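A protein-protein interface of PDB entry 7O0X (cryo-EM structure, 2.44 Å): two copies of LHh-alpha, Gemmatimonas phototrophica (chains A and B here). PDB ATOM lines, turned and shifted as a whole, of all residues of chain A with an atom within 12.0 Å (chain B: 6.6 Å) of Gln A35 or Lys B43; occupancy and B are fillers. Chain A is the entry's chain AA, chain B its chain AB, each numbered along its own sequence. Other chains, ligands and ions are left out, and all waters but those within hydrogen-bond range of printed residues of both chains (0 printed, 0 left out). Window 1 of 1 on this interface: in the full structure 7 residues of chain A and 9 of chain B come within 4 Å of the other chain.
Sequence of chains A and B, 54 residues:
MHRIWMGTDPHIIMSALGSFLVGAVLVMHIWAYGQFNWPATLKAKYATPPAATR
OG1 of Thr A41 sits at hydrogen-bond distance from O of Asn A37, 3.3 Å away.
The backbone carbonyl oxygen (O) of Tyr B46 sits at hydrogen-bond distance from the side-chain amide nitrogen (ND2) of Asn A37 (3.0 Å). The side-chain amide nitrogen (ND2) of Asn A37 lies within hydrogen-bond range of the side-chain hydroxyl (OG1) of Thr B48, 3.1 Å away.
Hydrophobic or aromatic side chains of chain B that line the printed part of chain A: Pro B39, Leu B42 and Tyr B46. Printed residues of chain A that touch a printed residue of chain B: Trp A31, Gln A35, Phe A36 and Asn A37. Hydrophobic or aromatic side chains of chain A that line the printed part of chain B: Trp A31 and Phe A36. Among the printed residues, no Asp or Glu carboxylate lies within 4 Å of a Lys or Arg side-chain nitrogen of the other chain.
Positions printed for both chains: 39, 40, 41 and 42. Of the 8 pairs that touch across the chains among the printed residues, none has its exchanged pair printed and touching as well.
Of the printed residues of chain B, Gln A35 touches Pro B39 (3.5 Å), Leu B42 (3.8 Å) and Lys B43 (3.4 Å). Lys B43 touches just one residue of chain A: Gln A35 (3.4 Å). No residue of chain A comes within 4 Å of Ala B40. Thr B41 touches none of the printed residues of chain A. Of the printed residues of chain A, Leu B42 touches Gln A35 and Phe A36. No residue of chain A comes within 4 Å of Ala B44. No residue of chain A comes within 4 Å of Lys B45. Printed residues of chain A within 4 Å of Tyr B46: Phe A36 (3.9 Å) and Asn A37 (3.0 Å). Of the printed residues of chain B, Asn A37 touches Tyr B46 and Thr B48. Printed residues of chain B within 4 Å of Phe A36: Leu B42 and Tyr B46. Trp A38 touches none of the printed residues of chain B. The nearest residue of chain B that does not touch Gln A35 is Tyr B46 (4.5 Å). The nearest printed residue of chain A that does not touch Tyr B46 is Gln A35 (4.5 Å).
Among the printed residues, pairs that only touch across the chains: Trp A31 with Pro B39 (3.7 Å), Gln A35 with Pro B39 (3.5 Å), Gln A35 with Leu B42 (3.8 Å), Gln A35 with Lys B43 (3.4 Å), Phe A36 with Leu B42 (3.9 Å) and Phe A36 with Tyr B46 (3.9 Å).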
ATOM      1  N   LEU A  26      14.004 -19.451   0.040  1.00  0.00           N
ATOM      2  CA  LEU A  26      15.277 -19.922   0.585  1.00  0.00           C
ATOM      3  C   LEU A  26      15.302 -19.846   2.107  1.00  0.00           C
ATOM      4  O   LEU A  26      15.687 -20.809   2.779  1.00  0.00           O
ATOM      5  CB  LEU A  26      16.440 -19.126  -0.005  1.00  0.00           C
ATOM      6  CG  LEU A  26      16.873 -19.482  -1.425  1.00  0.00           C
ATOM      7  CD1 LEU A  26      17.924 -18.506  -1.918  1.00  0.00           C
ATOM      8  CD2 LEU A  26      17.406 -20.902  -1.470  1.00  0.00           C
ATOM      9  N   VAL A  27      14.914 -18.700   2.668  1.00  0.00           N
ATOM     10  CA  VAL A  27      14.849 -18.561   4.122  1.00  0.00           C
ATOM     11  C   VAL A  27      13.933 -19.621   4.723  1.00  0.00           C
ATOM     12  O   VAL A  27      14.272 -20.268   5.720  1.00  0.00           O
ATOM     13  CB  VAL A  27      14.396 -17.141   4.506  1.00  0.00           C
ATOM     14  CG1 VAL A  27      14.037 -17.074   5.982  1.00  0.00           C
ATOM     15  CG2 VAL A  27      15.488 -16.137   4.188  1.00  0.00           C
ATOM     16  N   MET A  28      12.757 -19.811   4.122  1.00  0.00           N
ATOM     17  CA  MET A  28      11.786 -20.758   4.660  1.00  0.00           C
ATOM     18  C   MET A  28      12.308 -22.193   4.672  1.00  0.00           C
ATOM     19  O   MET A  28      12.081 -22.928   5.638  1.00  0.00           O
ATOM     20  CB  MET A  28      10.485 -20.673   3.860  1.00  0.00           C
ATOM     21  CG  MET A  28       9.610 -19.483   4.223  1.00  0.00           C
ATOM     22  SD  MET A  28       9.347 -19.283   5.995  1.00  0.00           S
ATOM     23  CE  MET A  28       8.805 -20.927   6.446  1.00  0.00           C
ATOM     24  N   HIS A  29      13.017 -22.610   3.619  1.00  0.00           N
ATOM     25  CA  HIS A  29      13.567 -23.965   3.601  1.00  0.00           C
ATOM     26  C   HIS A  29      14.709 -24.151   4.594  1.00  0.00           C
ATOM     27  O   HIS A  29      14.771 -25.182   5.271  1.00  0.00           O
ATOM     28  CB  HIS A  29      13.991 -24.359   2.188  1.00  0.00           C
ATOM     29  CG  HIS A  29      12.840 -24.699   1.293  1.00  0.00           C
ATOM     30  ND1 HIS A  29      11.990 -23.751   0.765  1.00  0.00           N
ATOM     31  CD2 HIS A  29      12.378 -25.898   0.863  1.00  0.00           C
ATOM     32  CE1 HIS A  29      11.066 -24.351   0.034  1.00  0.00           C
ATOM     33  NE2 HIS A  29      11.278 -25.654   0.078  1.00  0.00           N
ATOM     34  N   ILE A  30      15.628 -23.187   4.695  1.00  0.00           N
ATOM     35  CA  ILE A  30      16.704 -23.311   5.679  1.00  0.00           C
ATOM     36  C   ILE A  30      16.116 -23.441   7.076  1.00  0.00           C
ATOM     37  O   ILE A  30      16.520 -24.300   7.867  1.00  0.00           O
ATOM     38  CB  ILE A  30      17.664 -22.109   5.598  1.00  0.00           C
ATOM     39  CG1 ILE A  30      18.332 -22.019   4.229  1.00  0.00           C
ATOM     40  CG2 ILE A  30      18.717 -22.199   6.690  1.00  0.00           C
ATOM     41  CD1 ILE A  30      18.934 -20.658   3.961  1.00  0.00           C
ATOM     42  N   TRP A  31      15.150 -22.582   7.392  1.00  0.00           N
ATOM     43  CA  TRP A  31      14.456 -22.643   8.672  1.00  0.00           C
ATOM     44  C   TRP A  31      13.766 -23.993   8.864  1.00  0.00           C
ATOM     45  O   TRP A  31      13.976 -24.670   9.875  1.00  0.00           O
ATOM     46  CB  TRP A  31      13.462 -21.482   8.750  1.00  0.00           C
ATOM     47  CG  TRP A  31      12.649 -21.403   9.998  1.00  0.00           C
ATOM     48  CD1 TRP A  31      12.991 -20.770  11.154  1.00  0.00           C
ATOM     49  CD2 TRP A  31      11.335 -21.930  10.201  1.00  0.00           C
ATOM     50  NE1 TRP A  31      11.983 -20.891  12.076  1.00  0.00           N
ATOM     51  CE2 TRP A  31      10.952 -21.598  11.515  1.00  0.00           C
ATOM     52  CE3 TRP A  31      10.449 -22.661   9.406  1.00  0.00           C
ATOM     53  CZ2 TRP A  31       9.723 -21.972  12.050  1.00  0.00           C
ATOM     54  CZ3 TRP A  31       9.230 -23.032   9.940  1.00  0.00           C
ATOM     55  CH2 TRP A  31       8.878 -22.686  11.249  1.00  0.00           C
ATOM     56  N   ALA A  32      12.943 -24.399   7.892  1.00  0.00           N
ATOM     57  CA  ALA A  32      12.201 -25.657   7.994  1.00  0.00           C
ATOM     58  C   ALA A  32      13.113 -26.878   8.100  1.00  0.00           C
ATOM     59  O   ALA A  32      12.806 -27.816   8.844  1.00  0.00           O
ATOM     60  CB  ALA A  32      11.257 -25.803   6.802  1.00  0.00           C
ATOM     61  N   TYR A  33      14.231 -26.902   7.363  1.00  0.00           N
ATOM     62  CA  TYR A  33      15.158 -28.026   7.511  1.00  0.00           C
ATOM     63  C   TYR A  33      15.705 -28.128   8.927  1.00  0.00           C
ATOM     64  O   TYR A  33      15.984 -29.232   9.407  1.00  0.00           O
ATOM     65  CB  TYR A  33      16.334 -27.917   6.538  1.00  0.00           C
ATOM     66  CG  TYR A  33      16.013 -27.980   5.063  1.00  0.00           C
ATOM     67  CD1 TYR A  33      14.856 -28.586   4.600  1.00  0.00           C
ATOM     68  CD2 TYR A  33      16.904 -27.471   4.129  1.00  0.00           C
ATOM     69  CE1 TYR A  33      14.574 -28.641   3.248  1.00  0.00           C
ATOM     70  CE2 TYR A  33      16.639 -27.534   2.780  1.00  0.00           C
ATOM     71  CZ  TYR A  33      15.473 -28.116   2.344  1.00  0.00           C
ATOM     72  OH  TYR A  33      15.220 -28.191   0.996  1.00  0.00           O
ATOM     73  N   GLY A  34      15.866 -27.000   9.605  1.00  0.00           N
ATOM     74  CA  GLY A  34      16.200 -27.001  11.012  1.00  0.00           C
ATOM     75  C   GLY A  34      15.118 -27.577  11.900  1.00  0.00           C
ATOM     76  O   GLY A  34      15.360 -28.527  12.649  1.00  0.00           O
ATOM     77  N   GLN A  35      13.915 -27.006  11.819  1.00  0.00           N
ATOM     78  CA  GLN A  35      12.860 -27.355  12.765  1.00  0.00           C
ATOM     79  C   GLN A  35      12.318 -28.766  12.541  1.00  0.00           C
ATOM     80  O   GLN A  35      12.020 -29.475  13.509  1.00  0.00           O
ATOM     81  CB  GLN A  35      11.722 -26.336  12.681  1.00  0.00           C
ATOM     82  CG  GLN A  35      12.144 -24.872  12.759  1.00  0.00           C
ATOM     83  CD  GLN A  35      13.256 -24.615  13.758  1.00  0.00           C
ATOM     84  OE1 GLN A  35      14.385 -24.305  13.381  1.00  0.00           O
ATOM     85  NE2 GLN A  35      12.942 -24.744  15.039  1.00  0.00           N
ATOM     86  N   PHE A  36      12.175 -29.196  11.289  1.00  0.00           N
ATOM     87  CA  PHE A  36      11.556 -30.489  11.008  1.00  0.00           C
ATOM     88  C   PHE A  36      12.525 -31.667  11.021  1.00  0.00           C
ATOM     89  O   PHE A  36      12.084 -32.803  10.816  1.00  0.00           O
ATOM     90  CB  PHE A  36      10.800 -30.432   9.681  1.00  0.00           C
ATOM     91  CG  PHE A  36       9.518 -29.665   9.770  1.00  0.00           C
ATOM     92  CD1 PHE A  36       9.516 -28.284   9.696  1.00  0.00           C
ATOM     93  CD2 PHE A  36       8.319 -30.322   9.981  1.00  0.00           C
ATOM     94  CE1 PHE A  36       8.339 -27.575   9.800  1.00  0.00           C
ATOM     95  CE2 PHE A  36       7.138 -29.617  10.087  1.00  0.00           C
ATOM     96  CZ  PHE A  36       7.148 -28.243   9.997  1.00  0.00           C
ATOM     97  N   ASN A  37      13.818 -31.432  11.244  1.00  0.00           N
ATOM     98  CA  ASN A  37      14.831 -32.492  11.264  1.00  0.00           C
ATOM     99  C   ASN A  37      14.866 -33.304   9.967  1.00  0.00           C
ATOM    100  O   ASN A  37      15.142 -34.505   9.980  1.00  0.00           O
ATOM    101  CB  ASN A  37      14.620 -33.406  12.479  1.00  0.00           C
ATOM    102  CG  ASN A  37      15.830 -34.259  12.792  1.00  0.00           C
ATOM    103  OD1 ASN A  37      16.970 -33.838  12.598  1.00  0.00           O
ATOM    104  ND2 ASN A  37      15.590 -35.460  13.303  1.00  0.00           N
ATOM    105  N   TRP A  38      14.575 -32.665   8.836  1.00  0.00           N
ATOM    106  CA  TRP A  38      14.694 -33.275   7.521  1.00  0.00           C
ATOM    107  C   TRP A  38      15.491 -32.322   6.639  1.00  0.00           C
ATOM    108  O   TRP A  38      15.256 -31.110   6.689  1.00  0.00           O
ATOM    109  CB  TRP A  38      13.314 -33.537   6.896  1.00  0.00           C
ATOM    110  CG  TRP A  38      13.342 -34.323   5.610  1.00  0.00           C
ATOM    111  CD1 TRP A  38      13.107 -35.659   5.475  1.00  0.00           C
ATOM    112  CD2 TRP A  38      13.626 -33.834   4.291  1.00  0.00           C
ATOM    113  NE1 TRP A  38      13.220 -36.032   4.161  1.00  0.00           N
ATOM    114  CE2 TRP A  38      13.539 -34.932   3.413  1.00  0.00           C
ATOM    115  CE3 TRP A  38      13.945 -32.577   3.768  1.00  0.00           C
ATOM    116  CZ2 TRP A  38      13.759 -34.812   2.045  1.00  0.00           C
ATOM    117  CZ3 TRP A  38      14.166 -32.463   2.409  1.00  0.00           C
ATOM    118  CH2 TRP A  38      14.070 -33.574   1.565  1.00  0.00           C
ATOM    119  N   PRO A  39      16.436 -32.816   5.823  1.00  0.00           N
ATOM    120  CA  PRO A  39      16.798 -34.179   5.423  1.00  0.00           C
ATOM    121  C   PRO A  39      17.695 -34.942   6.391  1.00  0.00           C
ATOM    122  O   PRO A  39      18.240 -35.970   5.998  1.00  0.00           O
ATOM    123  CB  PRO A  39      17.532 -33.947   4.102  1.00  0.00           C
ATOM    124  CG  PRO A  39      18.264 -32.692   4.359  1.00  0.00           C
ATOM    125  CD  PRO A  39      17.244 -31.832   5.081  1.00  0.00           C
ATOM    126  N   ALA A  40      17.879 -34.443   7.614  1.00  0.00           N
ATOM    127  CA  ALA A  40      18.779 -35.115   8.545  1.00  0.00           C
ATOM    128  C   ALA A  40      18.330 -36.545   8.839  1.00  0.00           C
ATOM    129  O   ALA A  40      19.167 -37.444   8.976  1.00  0.00           O
ATOM    130  CB  ALA A  40      18.890 -34.309   9.839  1.00  0.00           C
ATOM    131  N   THR A  41      17.018 -36.779   8.934  1.00  0.00           N
ATOM    132  CA  THR A  41      16.517 -38.150   9.014  1.00  0.00           C
ATOM    133  C   THR A  41      16.647 -38.905   7.695  1.00  0.00           C
ATOM    134  O   THR A  41      16.781 -40.134   7.705  1.00  0.00           O
ATOM    135  CB  THR A  41      15.060 -38.165   9.484  1.00  0.00           C
ATOM    136  OG1 THR A  41      14.259 -37.354   8.616  1.00  0.00           O
ATOM    137  CG2 THR A  41      14.948 -37.656  10.911  1.00  0.00           C
ATOM    138  N   LEU A  42      16.605 -38.207   6.559  1.00  0.00           N
ATOM    139  CA  LEU A  42      16.853 -38.862   5.275  1.00  0.00           C
ATOM    140  C   LEU A  42      18.283 -39.377   5.178  1.00  0.00           C
ATOM    141  O   LEU A  42      18.518 -40.504   4.729  1.00  0.00           O
ATOM    142  CB  LEU A  42      16.548 -37.901   4.125  1.00  0.00           C
ATOM    143  CG  LEU A  42      17.119 -38.280   2.757  1.00  0.00           C
ATOM    144  CD1 LEU A  42      16.478 -39.551   2.233  1.00  0.00           C
ATOM    145  CD2 LEU A  42      16.941 -37.144   1.763  1.00  0.00           C
ATOM    146  N   PRO B  39       8.774 -22.095  17.289  1.00  0.00           N
ATOM    147  CA  PRO B  39       8.885 -23.514  16.930  1.00  0.00           C
ATOM    148  C   PRO B  39       9.743 -24.402  17.838  1.00  0.00           C
ATOM    149  O   PRO B  39      10.030 -25.528  17.438  1.00  0.00           O
ATOM    150  CB  PRO B  39       9.506 -23.441  15.534  1.00  0.00           C
ATOM    151  CG  PRO B  39      10.453 -22.317  15.666  1.00  0.00           C
ATOM    152  CD  PRO B  39       9.655 -21.279  16.433  1.00  0.00           C
ATOM    153  N   ALA B  40      10.163 -23.916  19.008  1.00  0.00           N
ATOM    154  CA  ALA B  40      11.023 -24.721  19.875  1.00  0.00           C
ATOM    155  C   ALA B  40      10.376 -26.043  20.289  1.00  0.00           C
ATOM    156  O   ALA B  40      11.060 -27.071  20.360  1.00  0.00           O
ATOM    157  CB  ALA B  40      11.416 -23.914  21.110  1.00  0.00           C
ATOM    158  N   THR B  41       9.069 -26.051  20.567  1.00  0.00           N
ATOM    159  CA  THR B  41       8.393 -27.327  20.806  1.00  0.00           C
ATOM    160  C   THR B  41       8.290 -28.178  19.546  1.00  0.00           C
ATOM    161  O   THR B  41       8.359 -29.410  19.628  1.00  0.00           O
ATOM    162  CB  THR B  41       6.998 -27.106  21.396  1.00  0.00           C
ATOM    163  OG1 THR B  41       6.223 -26.278  20.521  1.00  0.00           O
ATOM    164  CG2 THR B  41       7.087 -26.463  22.771  1.00  0.00           C
ATOM    165  N   LEU B  42       8.121 -27.550  18.381  1.00  0.00           N
ATOM    166  CA  LEU B  42       8.133 -28.288  17.120  1.00  0.00           C
ATOM    167  C   LEU B  42       9.465 -28.995  16.900  1.00  0.00           C
ATOM    168  O   LEU B  42       9.502 -30.186  16.574  1.00  0.00           O
ATOM    169  CB  LEU B  42       7.817 -27.345  15.959  1.00  0.00           C
ATOM    170  CG  LEU B  42       8.241 -27.796  14.560  1.00  0.00           C
ATOM    171  CD1 LEU B  42       7.449 -29.015  14.125  1.00  0.00           C
ATOM    172  CD2 LEU B  42       8.068 -26.665  13.561  1.00  0.00           C
ATOM    173  N   LYS B  43      10.572 -28.269  17.061  1.00  0.00           N
ATOM    174  CA  LYS B  43      11.890 -28.861  16.859  1.00  0.00           C
ATOM    175  C   LYS B  43      12.132 -30.024  17.814  1.00  0.00           C
ATOM    176  O   LYS B  43      12.645 -31.072  17.408  1.00  0.00           O
ATOM    177  CB  LYS B  43      12.968 -27.789  17.022  1.00  0.00           C
ATOM    178  CG  LYS B  43      14.386 -28.283  16.811  1.00  0.00           C
ATOM    179  CD  LYS B  43      15.381 -27.140  16.927  1.00  0.00           C
ATOM    180  CE  LYS B  43      16.801 -27.650  17.097  1.00  0.00           C
ATOM    181  NZ  LYS B  43      17.003 -28.315  18.414  1.00  0.00           N
ATOM    182  N   ALA B  44      11.775 -29.854  19.088  1.00  0.00           N
ATOM    183  CA  ALA B  44      11.908 -30.935  20.060  1.00  0.00           C
ATOM    184  C   ALA B  44      11.062 -32.153  19.701  1.00  0.00           C
ATOM    185  O   ALA B  44      11.456 -33.286  19.995  1.00  0.00           O
ATOM    186  CB  ALA B  44      11.537 -30.431  21.454  1.00  0.00           C
ATOM    187  N   LYS B  45       9.900 -31.943  19.075  1.00  0.00           N
ATOM    188  CA  LYS B  45       9.045 -33.065  18.685  1.00  0.00           C
ATOM    189  C   LYS B  45       9.745 -34.026  17.727  1.00  0.00           C
ATOM    190  O   LYS B  45       9.622 -35.247  17.870  1.00  0.00           O
ATOM    191  CB  LYS B  45       7.754 -32.546  18.048  1.00  0.00           C
ATOM    192  CG  LYS B  45       6.666 -33.602  17.926  1.00  0.00           C
ATOM    193  CD  LYS B  45       5.457 -33.101  17.148  1.00  0.00           C
ATOM    194  CE  LYS B  45       4.752 -31.953  17.852  1.00  0.00           C
ATOM    195  NZ  LYS B  45       3.423 -31.674  17.236  1.00  0.00           N
ATOM    196  N   TYR B  46      10.470 -33.501  16.742  1.00  0.00           N
ATOM    197  CA  TYR B  46      11.082 -34.325  15.706  1.00  0.00           C
ATOM    198  C   TYR B  46      12.591 -34.491  15.844  1.00  0.00           C
ATOM    199  O   TYR B  46      13.197 -35.177  15.015  1.00  0.00           O
ATOM    200  CB  TYR B  46      10.732 -33.758  14.327  1.00  0.00           C
ATOM    201  CG  TYR B  46       9.245 -33.792  14.058  1.00  0.00           C
ATOM    202  CD1 TYR B  46       8.576 -35.001  13.935  1.00  0.00           C
ATOM    203  CD2 TYR B  46       8.507 -32.621  13.965  1.00  0.00           C
ATOM    204  CE1 TYR B  46       7.216 -35.044  13.700  1.00  0.00           C
ATOM    205  CE2 TYR B  46       7.144 -32.655  13.734  1.00  0.00           C
ATOM    206  CZ  TYR B  46       6.506 -33.869  13.602  1.00  0.00           C
ATOM    207  OH  TYR B  46       5.150 -33.910  13.378  1.00  0.00           O
ATOM    208  N   ALA B  47      13.215 -33.878  16.847  1.00  0.00           N
ATOM    209  CA  ALA B  47      14.644 -34.052  17.070  1.00  0.00           C
ATOM    210  C   ALA B  47      14.999 -35.520  17.317  1.00  0.00           C
ATOM    211  O   ALA B  47      14.157 -36.342  17.690  1.00  0.00           O
ATOM    212  CB  ALA B  47      15.106 -33.202  18.252  1.00  0.00           C
ATOM    213  N   THR B  48      16.277 -35.841  17.099  1.00  0.00           N
ATOM    214  CA  THR B  48      16.830 -37.168  17.326  1.00  0.00           C
ATOM    215  C   THR B  48      17.683 -37.175  18.585  1.00  0.00           C
ATOM    216  O   THR B  48      18.557 -36.310  18.731  1.00  0.00           O
ATOM    217  CB  THR B  48      17.676 -37.608  16.123  1.00  0.00           C
ATOM    218  OG1 THR B  48      16.837 -37.753  14.971  1.00  0.00           O
ATOM    219  CG2 THR B  48      18.379 -38.927  16.407  1.00  0.00           C
